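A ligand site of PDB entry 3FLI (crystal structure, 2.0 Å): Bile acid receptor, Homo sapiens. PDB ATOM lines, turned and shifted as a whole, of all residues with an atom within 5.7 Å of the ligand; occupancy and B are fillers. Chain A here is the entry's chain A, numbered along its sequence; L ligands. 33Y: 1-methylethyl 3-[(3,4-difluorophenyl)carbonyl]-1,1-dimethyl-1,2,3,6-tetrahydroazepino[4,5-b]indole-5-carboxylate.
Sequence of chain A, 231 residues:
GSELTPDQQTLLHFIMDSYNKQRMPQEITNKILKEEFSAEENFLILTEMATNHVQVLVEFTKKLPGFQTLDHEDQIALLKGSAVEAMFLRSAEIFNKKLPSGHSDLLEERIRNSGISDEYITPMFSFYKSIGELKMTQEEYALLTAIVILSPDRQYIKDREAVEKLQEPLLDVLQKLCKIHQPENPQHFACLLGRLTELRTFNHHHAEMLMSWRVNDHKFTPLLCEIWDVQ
The side-chain hydroxyl (OH) of Tyr 128 is in hydrogen-bond range of an oxygen (O19) of the ligand, at 2.9 Å. N7 of the ligand sits close to O of Leu 46, at 3.4 Å. An oxygen (O17) of the ligand lies close to the side-chain hydroxyl (OG) of Ser 91 (3.4 Å). A nitrogen (N7) of the ligand sits close to the side-chain sulfur (SD) of Met 87 (3.7 Å). N of Ala 50 lies within hydrogen-bond range of O16 of the ligand (3.1 Å).
O of Thr 47 sits at hydrogen-bond distance from OG1 of Thr 51, 2.8 Å away. OG of Ser 91 sits at hydrogen-bond distance from O of Met 87 (2.9 Å). The side-chain hydroxyl of Tyr 128 lies within hydrogen-bond range of the side-chain sulfur of Met 124 (3.4 Å). The side-chain hydroxyl (OG1) of Thr 47 lies within hydrogen-bond range of the backbone carbonyl oxygen (O) of Phe 43, at 3.0 Å.
OG1 of Thr 29 lies close to F26 of the ligand, 3.3 Å away. An oxygen (O19) of the ligand lies close to the side-chain sulfur of Met 124, at 3.6 Å. Merely in contact with the ligand: Phe 95, Ile 32, Met 49, Ile 94, Ile 28, His 53, Ile 111, Met 209, Leu 107, Thr 47, Arg 90 and Phe 88. Within 4 Å of the ligand: Ile 28, Thr 29, Ile 32, Leu 46, Thr 47, Met 49, Ala 50, His 53, Met 87, Phe 88, Arg 90, Ser 91, Ile 94, Phe 95, Leu 107, Ile 111, Met 124, Tyr 128 and Met 209.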
ATOM      1  N   PRO A  25       6.482  34.146   5.497  1.00  0.00           N
ATOM      2  CA  PRO A  25       5.527  34.441   4.401  1.00  0.00           C
ATOM      3  C   PRO A  25       6.037  34.032   3.016  1.00  0.00           C
ATOM      4  O   PRO A  25       5.275  33.455   2.271  1.00  0.00           O
ATOM      5  CB  PRO A  25       5.315  35.951   4.520  1.00  0.00           C
ATOM      6  CG  PRO A  25       5.514  36.185   6.084  1.00  0.00           C
ATOM      7  CD  PRO A  25       6.667  35.302   6.407  1.00  0.00           C
ATOM      8  N   ILE A  28       5.778  30.385   1.944  1.00  0.00           N
ATOM      9  CA  ILE A  28       4.442  30.028   1.510  1.00  0.00           C
ATOM     10  C   ILE A  28       4.215  30.525   0.071  1.00  0.00           C
ATOM     11  O   ILE A  28       3.813  29.797  -0.841  1.00  0.00           O
ATOM     12  CB  ILE A  28       3.386  30.705   2.465  1.00  0.00           C
ATOM     13  CG1 ILE A  28       3.520  30.141   3.897  1.00  0.00           C
ATOM     14  CG2 ILE A  28       1.993  30.606   1.883  1.00  0.00           C
ATOM     15  CD1 ILE A  28       3.344  28.611   4.009  1.00  0.00           C
ATOM     16  N   THR A  29       4.593  31.774  -0.110  1.00  0.00           N
ATOM     17  CA  THR A  29       4.280  32.613  -1.246  1.00  0.00           C
ATOM     18  C   THR A  29       5.232  32.254  -2.466  1.00  0.00           C
ATOM     19  O   THR A  29       4.775  32.176  -3.618  1.00  0.00           O
ATOM     20  CB  THR A  29       4.328  34.039  -0.656  1.00  0.00           C
ATOM     21  OG1 THR A  29       3.018  34.631  -0.484  1.00  0.00           O
ATOM     22  CG2 THR A  29       5.315  34.897  -1.221  1.00  0.00           C
ATOM     23  N   ILE A  32       3.645  29.139  -4.259  1.00  0.00           N
ATOM     24  CA  ILE A  32       2.489  29.375  -5.113  1.00  0.00           C
ATOM     25  C   ILE A  32       2.885  30.147  -6.375  1.00  0.00           C
ATOM     26  O   ILE A  32       2.210  30.030  -7.398  1.00  0.00           O
ATOM     27  CB  ILE A  32       1.372  30.123  -4.327  1.00  0.00           C
ATOM     28  CG1 ILE A  32       0.853  29.251  -3.186  1.00  0.00           C
ATOM     29  CG2 ILE A  32       0.169  30.479  -5.256  1.00  0.00           C
ATOM     30  CD1 ILE A  32       0.031  30.012  -2.148  1.00  0.00           C
ATOM     31  N   PHE A  43      -3.672  23.023  -5.425  1.00  0.00           N
ATOM     32  CA  PHE A  43      -4.553  22.508  -4.381  1.00  0.00           C
ATOM     33  C   PHE A  43      -3.866  21.567  -3.382  1.00  0.00           C
ATOM     34  O   PHE A  43      -4.144  21.634  -2.178  1.00  0.00           O
ATOM     35  CB  PHE A  43      -5.782  21.787  -4.951  1.00  0.00           C
ATOM     36  CG  PHE A  43      -6.836  21.500  -3.926  1.00  0.00           C
ATOM     37  CD1 PHE A  43      -7.867  22.406  -3.693  1.00  0.00           C
ATOM     38  CD2 PHE A  43      -6.797  20.354  -3.171  1.00  0.00           C
ATOM     39  CE1 PHE A  43      -8.842  22.160  -2.735  1.00  0.00           C
ATOM     40  CE2 PHE A  43      -7.762  20.101  -2.193  1.00  0.00           C
ATOM     41  CZ  PHE A  43      -8.783  21.005  -1.979  1.00  0.00           C
ATOM     42  N   LEU A  46      -1.725  23.766  -1.175  1.00  0.00           N
ATOM     43  CA  LEU A  46      -2.561  24.394  -0.142  1.00  0.00           C
ATOM     44  C   LEU A  46      -2.963  23.442   0.972  1.00  0.00           C
ATOM     45  O   LEU A  46      -3.051  23.847   2.123  1.00  0.00           O
ATOM     46  CB  LEU A  46      -3.834  24.935  -0.795  1.00  0.00           C
ATOM     47  CG  LEU A  46      -3.632  26.198  -1.627  1.00  0.00           C
ATOM     48  CD1 LEU A  46      -4.970  26.512  -2.305  1.00  0.00           C
ATOM     49  CD2 LEU A  46      -3.145  27.370  -0.752  1.00  0.00           C
ATOM     50  N   THR A  47      -3.270  22.189   0.618  1.00  0.00           N
ATOM     51  CA  THR A  47      -3.570  21.172   1.622  1.00  0.00           C
ATOM     52  C   THR A  47      -2.360  20.929   2.548  1.00  0.00           C
ATOM     53  O   THR A  47      -2.506  20.780   3.810  1.00  0.00           O
ATOM     54  CB  THR A  47      -4.060  19.823   0.976  1.00  0.00           C
ATOM     55  OG1 THR A  47      -5.180  20.065   0.121  1.00  0.00           O
ATOM     56  CG2 THR A  47      -4.480  18.850   2.047  1.00  0.00           C
ATOM     57  N   MET A  49       0.142  23.116   3.123  1.00  0.00           N
ATOM     58  CA  MET A  49       0.292  24.339   3.931  1.00  0.00           C
ATOM     59  C   MET A  49      -0.727  24.427   5.058  1.00  0.00           C
ATOM     60  O   MET A  49      -0.403  24.926   6.125  1.00  0.00           O
ATOM     61  CB  MET A  49       0.132  25.586   3.060  1.00  0.00           C
ATOM     62  CG  MET A  49       1.202  25.777   2.048  1.00  0.00           C
ATOM     63  SD  MET A  49       0.763  27.090   0.867  1.00  0.00           S
ATOM     64  CE  MET A  49       2.344  27.239   0.119  1.00  0.00           C
ATOM     65  N   ALA A  50      -1.946  23.976   4.828  1.00  0.00           N
ATOM     66  CA  ALA A  50      -3.013  23.983   5.876  1.00  0.00           C
ATOM     67  C   ALA A  50      -2.651  23.001   7.004  1.00  0.00           C
ATOM     68  O   ALA A  50      -2.834  23.292   8.173  1.00  0.00           O
ATOM     69  CB  ALA A  50      -4.353  23.626   5.269  1.00  0.00           C
ATOM     70  N   THR A  51      -2.134  21.829   6.638  1.00  0.00           N
ATOM     71  CA  THR A  51      -1.676  20.829   7.585  1.00  0.00           C
ATOM     72  C   THR A  51      -0.517  21.330   8.453  1.00  0.00           C
ATOM     73  O   THR A  51      -0.525  21.166   9.650  1.00  0.00           O
ATOM     74  CB  THR A  51      -1.184  19.556   6.826  1.00  0.00           C
ATOM     75  OG1 THR A  51      -2.210  19.090   5.962  1.00  0.00           O
ATOM     76  CG2 THR A  51      -0.789  18.470   7.796  1.00  0.00           C
ATOM     77  N   HIS A  53       0.096  24.491   8.943  1.00  0.00           N
ATOM     78  CA  HIS A  53      -0.493  25.584   9.784  1.00  0.00           C
ATOM     79  C   HIS A  53      -1.122  24.996  11.055  1.00  0.00           C
ATOM     80  O   HIS A  53      -0.898  25.493  12.166  1.00  0.00           O
ATOM     81  CB  HIS A  53      -1.530  26.431   9.031  1.00  0.00           C
ATOM     82  CG  HIS A  53      -2.027  27.553   9.856  1.00  0.00           C
ATOM     83  ND1 HIS A  53      -3.078  27.417  10.730  1.00  0.00           N
ATOM     84  CD2 HIS A  53      -1.499  28.778  10.102  1.00  0.00           C
ATOM     85  CE1 HIS A  53      -3.224  28.537  11.415  1.00  0.00           C
ATOM     86  NE2 HIS A  53      -2.276  29.379  11.052  1.00  0.00           N
ATOM     87  N   MET A  87      -6.069  30.248  10.619  1.00  0.00           N
ATOM     88  CA  MET A  87      -5.522  30.079   9.269  1.00  0.00           C
ATOM     89  C   MET A  87      -5.812  31.298   8.374  1.00  0.00           C
ATOM     90  O   MET A  87      -4.923  31.824   7.679  1.00  0.00           O
ATOM     91  CB  MET A  87      -6.061  28.789   8.656  1.00  0.00           C
ATOM     92  CG  MET A  87      -5.439  28.452   7.349  1.00  0.00           C
ATOM     93  SD  MET A  87      -6.262  27.094   6.466  1.00  0.00           S
ATOM     94  CE  MET A  87      -7.867  27.757   6.060  1.00  0.00           C
ATOM     95  N   PHE A  88      -7.043  31.804   8.435  1.00  0.00           N
ATOM     96  CA  PHE A  88      -7.381  32.977   7.634  1.00  0.00           C
ATOM     97  C   PHE A  88      -6.681  34.276   8.087  1.00  0.00           C
ATOM     98  O   PHE A  88      -6.333  35.129   7.262  1.00  0.00           O
ATOM     99  CB  PHE A  88      -8.907  33.104   7.543  1.00  0.00           C
ATOM    100  CG  PHE A  88      -9.533  32.140   6.552  1.00  0.00           C
ATOM    101  CD1 PHE A  88      -9.363  32.313   5.195  1.00  0.00           C
ATOM    102  CD2 PHE A  88     -10.296  31.059   6.987  1.00  0.00           C
ATOM    103  CE1 PHE A  88      -9.951  31.408   4.285  1.00  0.00           C
ATOM    104  CE2 PHE A  88     -10.886  30.168   6.059  1.00  0.00           C
ATOM    105  CZ  PHE A  88     -10.693  30.342   4.739  1.00  0.00           C
ATOM    106  N   ARG A  90      -3.715  34.352   9.545  1.00  0.00           N
ATOM    107  CA  ARG A  90      -2.320  34.230   9.109  1.00  0.00           C
ATOM    108  C   ARG A  90      -2.209  34.457   7.609  1.00  0.00           C
ATOM    109  O   ARG A  90      -1.245  35.062   7.147  1.00  0.00           O
ATOM    110  CB  ARG A  90      -1.726  32.884   9.502  1.00  0.00           C
ATOM    111  CG  ARG A  90      -0.260  32.674   9.007  1.00  0.00           C
ATOM    112  CD  ARG A  90       0.696  33.664   9.586  1.00  0.00           C
ATOM    113  NE  ARG A  90       2.073  33.310   9.239  1.00  0.00           N
ATOM    114  CZ  ARG A  90       3.142  33.989   9.637  1.00  0.00           C
ATOM    115  NH1 ARG A  90       3.005  35.068  10.374  1.00  0.00           N
ATOM    116  NH2 ARG A  90       4.353  33.600   9.269  1.00  0.00           N
ATOM    117  N   SER A  91      -3.206  34.012   6.854  1.00  0.00           N
ATOM    118  CA  SER A  91      -3.244  34.262   5.398  1.00  0.00           C
ATOM    119  C   SER A  91      -3.307  35.753   5.078  1.00  0.00           C
ATOM    120  O   SER A  91      -2.602  36.233   4.182  1.00  0.00           O
ATOM    121  CB  SER A  91      -4.415  33.521   4.768  1.00  0.00           C
ATOM    122  OG  SER A  91      -4.180  32.128   4.928  1.00  0.00           O
ATOM    123  N   ALA A  92      -4.087  36.498   5.872  1.00  0.00           N
ATOM    124  CA  ALA A  92      -4.130  37.983   5.757  1.00  0.00           C
ATOM    125  C   ALA A  92      -2.730  38.591   5.999  1.00  0.00           C
ATOM    126  O   ALA A  92      -2.233  39.431   5.229  1.00  0.00           O
ATOM    127  CB  ALA A  92      -5.148  38.551   6.757  1.00  0.00           C
ATOM    128  N   ILE A  94       0.190  37.094   5.723  1.00  0.00           N
ATOM    129  CA  ILE A  94       1.078  36.669   4.640  1.00  0.00           C
ATOM    130  C   ILE A  94       0.811  37.513   3.397  1.00  0.00           C
ATOM    131  O   ILE A  94       1.734  38.079   2.796  1.00  0.00           O
ATOM    132  CB  ILE A  94       0.876  35.169   4.307  1.00  0.00           C
ATOM    133  CG1 ILE A  94       1.454  34.287   5.413  1.00  0.00           C
ATOM    134  CG2 ILE A  94       1.531  34.814   2.958  1.00  0.00           C
ATOM    135  CD1 ILE A  94       1.093  32.855   5.192  1.00  0.00           C
ATOM    136  N   PHE A  95      -0.476  37.663   3.069  1.00  0.00           N
ATOM    137  CA  PHE A  95      -0.884  38.264   1.813  1.00  0.00           C
ATOM    138  C   PHE A  95      -0.413  39.707   1.683  1.00  0.00           C
ATOM    139  O   PHE A  95      -0.097  40.142   0.560  1.00  0.00           O
ATOM    140  CB  PHE A  95      -2.398  38.179   1.620  1.00  0.00           C
ATOM    141  CG  PHE A  95      -2.892  38.827   0.354  1.00  0.00           C
ATOM    142  CD1 PHE A  95      -3.398  40.109   0.385  1.00  0.00           C
ATOM    143  CD2 PHE A  95      -2.824  38.163  -0.866  1.00  0.00           C
ATOM    144  CE1 PHE A  95      -3.823  40.732  -0.781  1.00  0.00           C
ATOM    145  CE2 PHE A  95      -3.253  38.800  -2.049  1.00  0.00           C
ATOM    146  CZ  PHE A  95      -3.762  40.076  -2.000  1.00  0.00           C
ATOM    147  N   LEU A 107      -0.593  36.070  -7.274  1.00  0.00           N
ATOM    148  CA  LEU A 107      -0.931  35.235  -6.119  1.00  0.00           C
ATOM    149  C   LEU A 107      -2.464  35.004  -6.044  1.00  0.00           C
ATOM    150  O   LEU A 107      -2.944  33.871  -5.960  1.00  0.00           O
ATOM    151  CB  LEU A 107      -0.417  35.903  -4.842  1.00  0.00           C
ATOM    152  CG  LEU A 107      -0.667  35.145  -3.538  1.00  0.00           C
ATOM    153  CD1 LEU A 107      -0.167  33.692  -3.616  1.00  0.00           C
ATOM    154  CD2 LEU A 107      -0.041  35.861  -2.352  1.00  0.00           C
ATOM    155  N   ILE A 111      -4.674  31.442  -6.646  1.00  0.00           N
ATOM    156  CA  ILE A 111      -5.546  30.936  -5.608  1.00  0.00           C
ATOM    157  C   ILE A 111      -7.001  30.837  -6.116  1.00  0.00           C
ATOM    158  O   ILE A 111      -7.720  29.879  -5.781  1.00  0.00           O
ATOM    159  CB  ILE A 111      -5.431  31.777  -4.325  1.00  0.00           C
ATOM    160  CG1 ILE A 111      -4.163  31.333  -3.564  1.00  0.00           C
ATOM    161  CG2 ILE A 111      -6.657  31.621  -3.448  1.00  0.00           C
ATOM    162  CD1 ILE A 111      -3.748  32.251  -2.445  1.00  0.00           C
ATOM    163  N   ILE A 116     -11.367  25.917  -6.315  1.00  0.00           N
ATOM    164  CA  ILE A 116     -12.410  26.441  -5.420  1.00  0.00           C
ATOM    165  C   ILE A 116     -13.076  27.699  -5.975  1.00  0.00           C
ATOM    166  O   ILE A 116     -12.427  28.588  -6.571  1.00  0.00           O
ATOM    167  CB  ILE A 116     -11.951  26.626  -3.953  1.00  0.00           C
ATOM    168  CG1 ILE A 116     -12.801  27.691  -3.267  1.00  0.00           C
ATOM    169  CG2 ILE A 116     -10.453  26.955  -3.852  1.00  0.00           C
ATOM    170  CD1 ILE A 116     -12.400  27.990  -1.900  1.00  0.00           C
ATOM    171  N   ILE A 121     -13.742  32.586  -2.606  1.00  0.00           N
ATOM    172  CA  ILE A 121     -12.485  33.301  -2.772  1.00  0.00           C
ATOM    173  C   ILE A 121     -12.632  34.834  -2.687  1.00  0.00           C
ATOM    174  O   ILE A 121     -11.832  35.501  -2.033  1.00  0.00           O
ATOM    175  CB  ILE A 121     -11.752  32.860  -4.083  1.00  0.00           C
ATOM    176  CG1 ILE A 121     -11.498  31.335  -4.060  1.00  0.00           C
ATOM    177  CG2 ILE A 121     -10.450  33.601  -4.243  1.00  0.00           C
ATOM    178  CD1 ILE A 121     -10.748  30.839  -2.845  1.00  0.00           C
ATOM    179  N   MET A 124     -12.785  36.361   0.753  1.00  0.00           N
ATOM    180  CA  MET A 124     -11.587  36.154   1.495  1.00  0.00           C
ATOM    181  C   MET A 124     -10.511  37.212   1.068  1.00  0.00           C
ATOM    182  O   MET A 124      -9.921  37.832   1.935  1.00  0.00           O
ATOM    183  CB  MET A 124     -11.142  34.707   1.408  1.00  0.00           C
ATOM    184  CG  MET A 124     -10.085  34.410   0.443  1.00  0.00           C
ATOM    185  SD  MET A 124      -9.485  32.744   0.696  1.00  0.00           S
ATOM    186  CE  MET A 124     -10.908  31.689   0.749  1.00  0.00           C
ATOM    187  N   PHE A 125     -10.313  37.466  -0.224  1.00  0.00           N
ATOM    188  CA  PHE A 125      -9.371  38.537  -0.618  1.00  0.00           C
ATOM    189  C   PHE A 125      -9.831  39.941  -0.216  1.00  0.00           C
ATOM    190  O   PHE A 125      -8.997  40.778   0.094  1.00  0.00           O
ATOM    191  CB  PHE A 125      -8.957  38.434  -2.088  1.00  0.00           C
ATOM    192  CG  PHE A 125      -7.985  37.324  -2.370  1.00  0.00           C
ATOM    193  CD1 PHE A 125      -8.409  36.121  -2.911  1.00  0.00           C
ATOM    194  CD2 PHE A 125      -6.661  37.464  -2.065  1.00  0.00           C
ATOM    195  CE1 PHE A 125      -7.516  35.110  -3.163  1.00  0.00           C
ATOM    196  CE2 PHE A 125      -5.771  36.437  -2.312  1.00  0.00           C
ATOM    197  CZ  PHE A 125      -6.196  35.258  -2.835  1.00  0.00           C
ATOM    198  N   TYR A 128      -8.638  40.153   3.370  1.00  0.00           N
ATOM    199  CA  TYR A 128      -7.183  40.353   3.462  1.00  0.00           C
ATOM    200  C   TYR A 128      -6.770  41.806   3.207  1.00  0.00           C
ATOM    201  O   TYR A 128      -5.979  42.383   3.947  1.00  0.00           O
ATOM    202  CB  TYR A 128      -6.372  39.433   2.518  1.00  0.00           C
ATOM    203  CG  TYR A 128      -6.595  37.965   2.654  1.00  0.00           C
ATOM    204  CD1 TYR A 128      -6.352  37.110   1.561  1.00  0.00           C
ATOM    205  CD2 TYR A 128      -7.012  37.418   3.838  1.00  0.00           C
ATOM    206  CE1 TYR A 128      -6.594  35.728   1.648  1.00  0.00           C
ATOM    207  CE2 TYR A 128      -7.206  36.017   3.970  1.00  0.00           C
ATOM    208  CZ  TYR A 128      -7.006  35.207   2.863  1.00  0.00           C
ATOM    209  OH  TYR A 128      -7.220  33.883   2.996  1.00  0.00           O
ATOM    210  N   HIS A 206     -15.749  28.046   5.098  1.00  0.00           N
ATOM    211  CA  HIS A 206     -14.885  26.854   5.047  1.00  0.00           C
ATOM    212  C   HIS A 206     -15.684  25.539   5.106  1.00  0.00           C
ATOM    213  O   HIS A 206     -15.398  24.588   4.386  1.00  0.00           O
ATOM    214  CB  HIS A 206     -13.891  26.904   6.203  1.00  0.00           C
ATOM    215  CG  HIS A 206     -12.860  25.827   6.180  1.00  0.00           C
ATOM    216  ND1 HIS A 206     -11.690  25.946   5.462  1.00  0.00           N
ATOM    217  CD2 HIS A 206     -12.794  24.634   6.806  1.00  0.00           C
ATOM    218  CE1 HIS A 206     -10.949  24.871   5.654  1.00  0.00           C
ATOM    219  NE2 HIS A 206     -11.607  24.046   6.452  1.00  0.00           N
ATOM    220  N   MET A 209     -17.183  25.284   1.759  1.00  0.00           N
ATOM    221  CA  MET A 209     -16.088  24.986   0.832  1.00  0.00           C
ATOM    222  C   MET A 209     -15.657  23.517   0.875  1.00  0.00           C
ATOM    223  O   MET A 209     -15.519  22.882  -0.162  1.00  0.00           O
ATOM    224  CB  MET A 209     -14.897  25.879   1.154  1.00  0.00           C
ATOM    225  CG  MET A 209     -13.753  25.784   0.155  1.00  0.00           C
ATOM    226  SD  MET A 209     -12.081  25.740   0.880  1.00  0.00           S
ATOM    227  CE  MET A 209     -11.646  23.986   0.816  1.00  0.00           C
ATOM    228  N   PHE A 220      -8.241  14.245   2.765  1.00  0.00           N
ATOM    229  CA  PHE A 220      -7.321  15.163   3.430  1.00  0.00           C
ATOM    230  C   PHE A 220      -6.339  14.379   4.312  1.00  0.00           C
ATOM    231  O   PHE A 220      -6.477  13.140   4.487  1.00  0.00           O
ATOM    232  CB  PHE A 220      -8.106  16.208   4.250  1.00  0.00           C
ATOM    233  CG  PHE A 220      -8.926  17.171   3.384  1.00  0.00           C
ATOM    234  CD1 PHE A 220     -10.290  16.995   3.231  1.00  0.00           C
ATOM    235  CD2 PHE A 220      -8.295  18.197   2.681  1.00  0.00           C
ATOM    236  CE1 PHE A 220     -11.054  17.854   2.394  1.00  0.00           C
ATOM    237  CE2 PHE A 220      -9.022  19.063   1.842  1.00  0.00           C
ATOM    238  CZ  PHE A 220     -10.408  18.892   1.697  1.00  0.00           C
ATOM    239  N   TRP A 228     -10.050  19.452  11.648  1.00  0.00           N
ATOM    240  CA  TRP A 228     -11.224  19.922  10.903  1.00  0.00           C
ATOM    241  C   TRP A 228     -12.429  18.965  11.019  1.00  0.00           C
ATOM    242  O   TRP A 228     -13.563  19.370  10.774  1.00  0.00           O
ATOM    243  CB  TRP A 228     -10.931  20.064   9.419  1.00  0.00           C
ATOM    244  CG  TRP A 228     -10.052  21.213   9.029  1.00  0.00           C
ATOM    245  CD1 TRP A 228      -9.539  22.163   9.844  1.00  0.00           C
ATOM    246  CD2 TRP A 228      -9.553  21.492   7.715  1.00  0.00           C
ATOM    247  NE1 TRP A 228      -8.784  23.027   9.152  1.00  0.00           N
ATOM    248  CE2 TRP A 228      -8.761  22.650   7.827  1.00  0.00           C
ATOM    249  CE3 TRP A 228      -9.676  20.880   6.466  1.00  0.00           C
ATOM    250  CZ2 TRP A 228      -8.116  23.235   6.730  1.00  0.00           C
ATOM    251  CZ3 TRP A 228      -9.036  21.463   5.357  1.00  0.00           C
ATOM    252  CH2 TRP A 228      -8.256  22.618   5.498  1.00  0.00           C
HETATM  253  F32 33Y L   1      -1.716  35.042   0.811  1.00  0.00           F
HETATM  254  C24 33Y L   1      -2.076  33.808   0.840  1.00  0.00           C
HETATM  255  C23 33Y L   1      -1.110  32.840   0.562  1.00  0.00           C
HETATM  256  F26 33Y L   1       0.141  33.090   0.269  1.00  0.00           F
HETATM  257  C22 33Y L   1      -1.433  31.524   0.559  1.00  0.00           C
HETATM  258  C21 33Y L   1      -2.714  31.200   0.897  1.00  0.00           C
HETATM  259  C25 33Y L   1      -3.409  33.497   1.151  1.00  0.00           C
HETATM  260  C20 33Y L   1      -3.704  32.152   1.229  1.00  0.00           C
HETATM  261  C18 33Y L   1      -5.092  31.726   1.383  1.00  0.00           C
HETATM  262  O19 33Y L   1      -5.925  32.395   0.823  1.00  0.00           O
HETATM  263  N12 33Y L   1      -5.371  30.523   1.952  1.00  0.00           N
HETATM  264  C13 33Y L   1      -6.774  30.129   1.847  1.00  0.00           C
HETATM  265  C14 33Y L   1      -7.318  28.853   1.280  1.00  0.00           C
HETATM  266  C27 33Y L   1      -8.827  28.689   1.630  1.00  0.00           C
HETATM  267  C28 33Y L   1      -7.170  29.130  -0.239  1.00  0.00           C
HETATM  268  C9  33Y L   1      -6.553  27.688   1.874  1.00  0.00           C
HETATM  269  C5  33Y L   1      -6.911  26.344   1.555  1.00  0.00           C
HETATM  270  C6  33Y L   1      -7.910  25.711   0.714  1.00  0.00           C
HETATM  271  C1  33Y L   1      -8.011  24.323   0.621  1.00  0.00           C
HETATM  272  C11 33Y L   1      -4.476  29.725   2.631  1.00  0.00           C
HETATM  273  C10 33Y L   1      -4.615  28.546   3.299  1.00  0.00           C
HETATM  274  C15 33Y L   1      -3.434  27.978   4.023  1.00  0.00           C
HETATM  275  O17 33Y L   1      -2.931  29.004   4.818  1.00  0.00           O
HETATM  276  C29 33Y L   1      -1.681  28.901   5.531  1.00  0.00           C
HETATM  277  C31 33Y L   1      -0.493  29.316   4.671  1.00  0.00           C
HETATM  278  C30 33Y L   1      -1.771  29.846   6.725  1.00  0.00           C
HETATM  279  O16 33Y L   1      -3.079  26.823   4.276  1.00  0.00           O
HETATM  280  C8  33Y L   1      -5.604  27.710   2.970  1.00  0.00           C
HETATM  281  N7  33Y L   1      -5.227  26.338   2.960  1.00  0.00           N
HETATM  282  C4  33Y L   1      -6.063  25.498   2.273  1.00  0.00           C
HETATM  283  C3  33Y L   1      -6.132  24.074   2.173  1.00  0.00           C
HETATM  284  C2  33Y L   1      -7.098  23.494   1.346  1.00  0.00           C
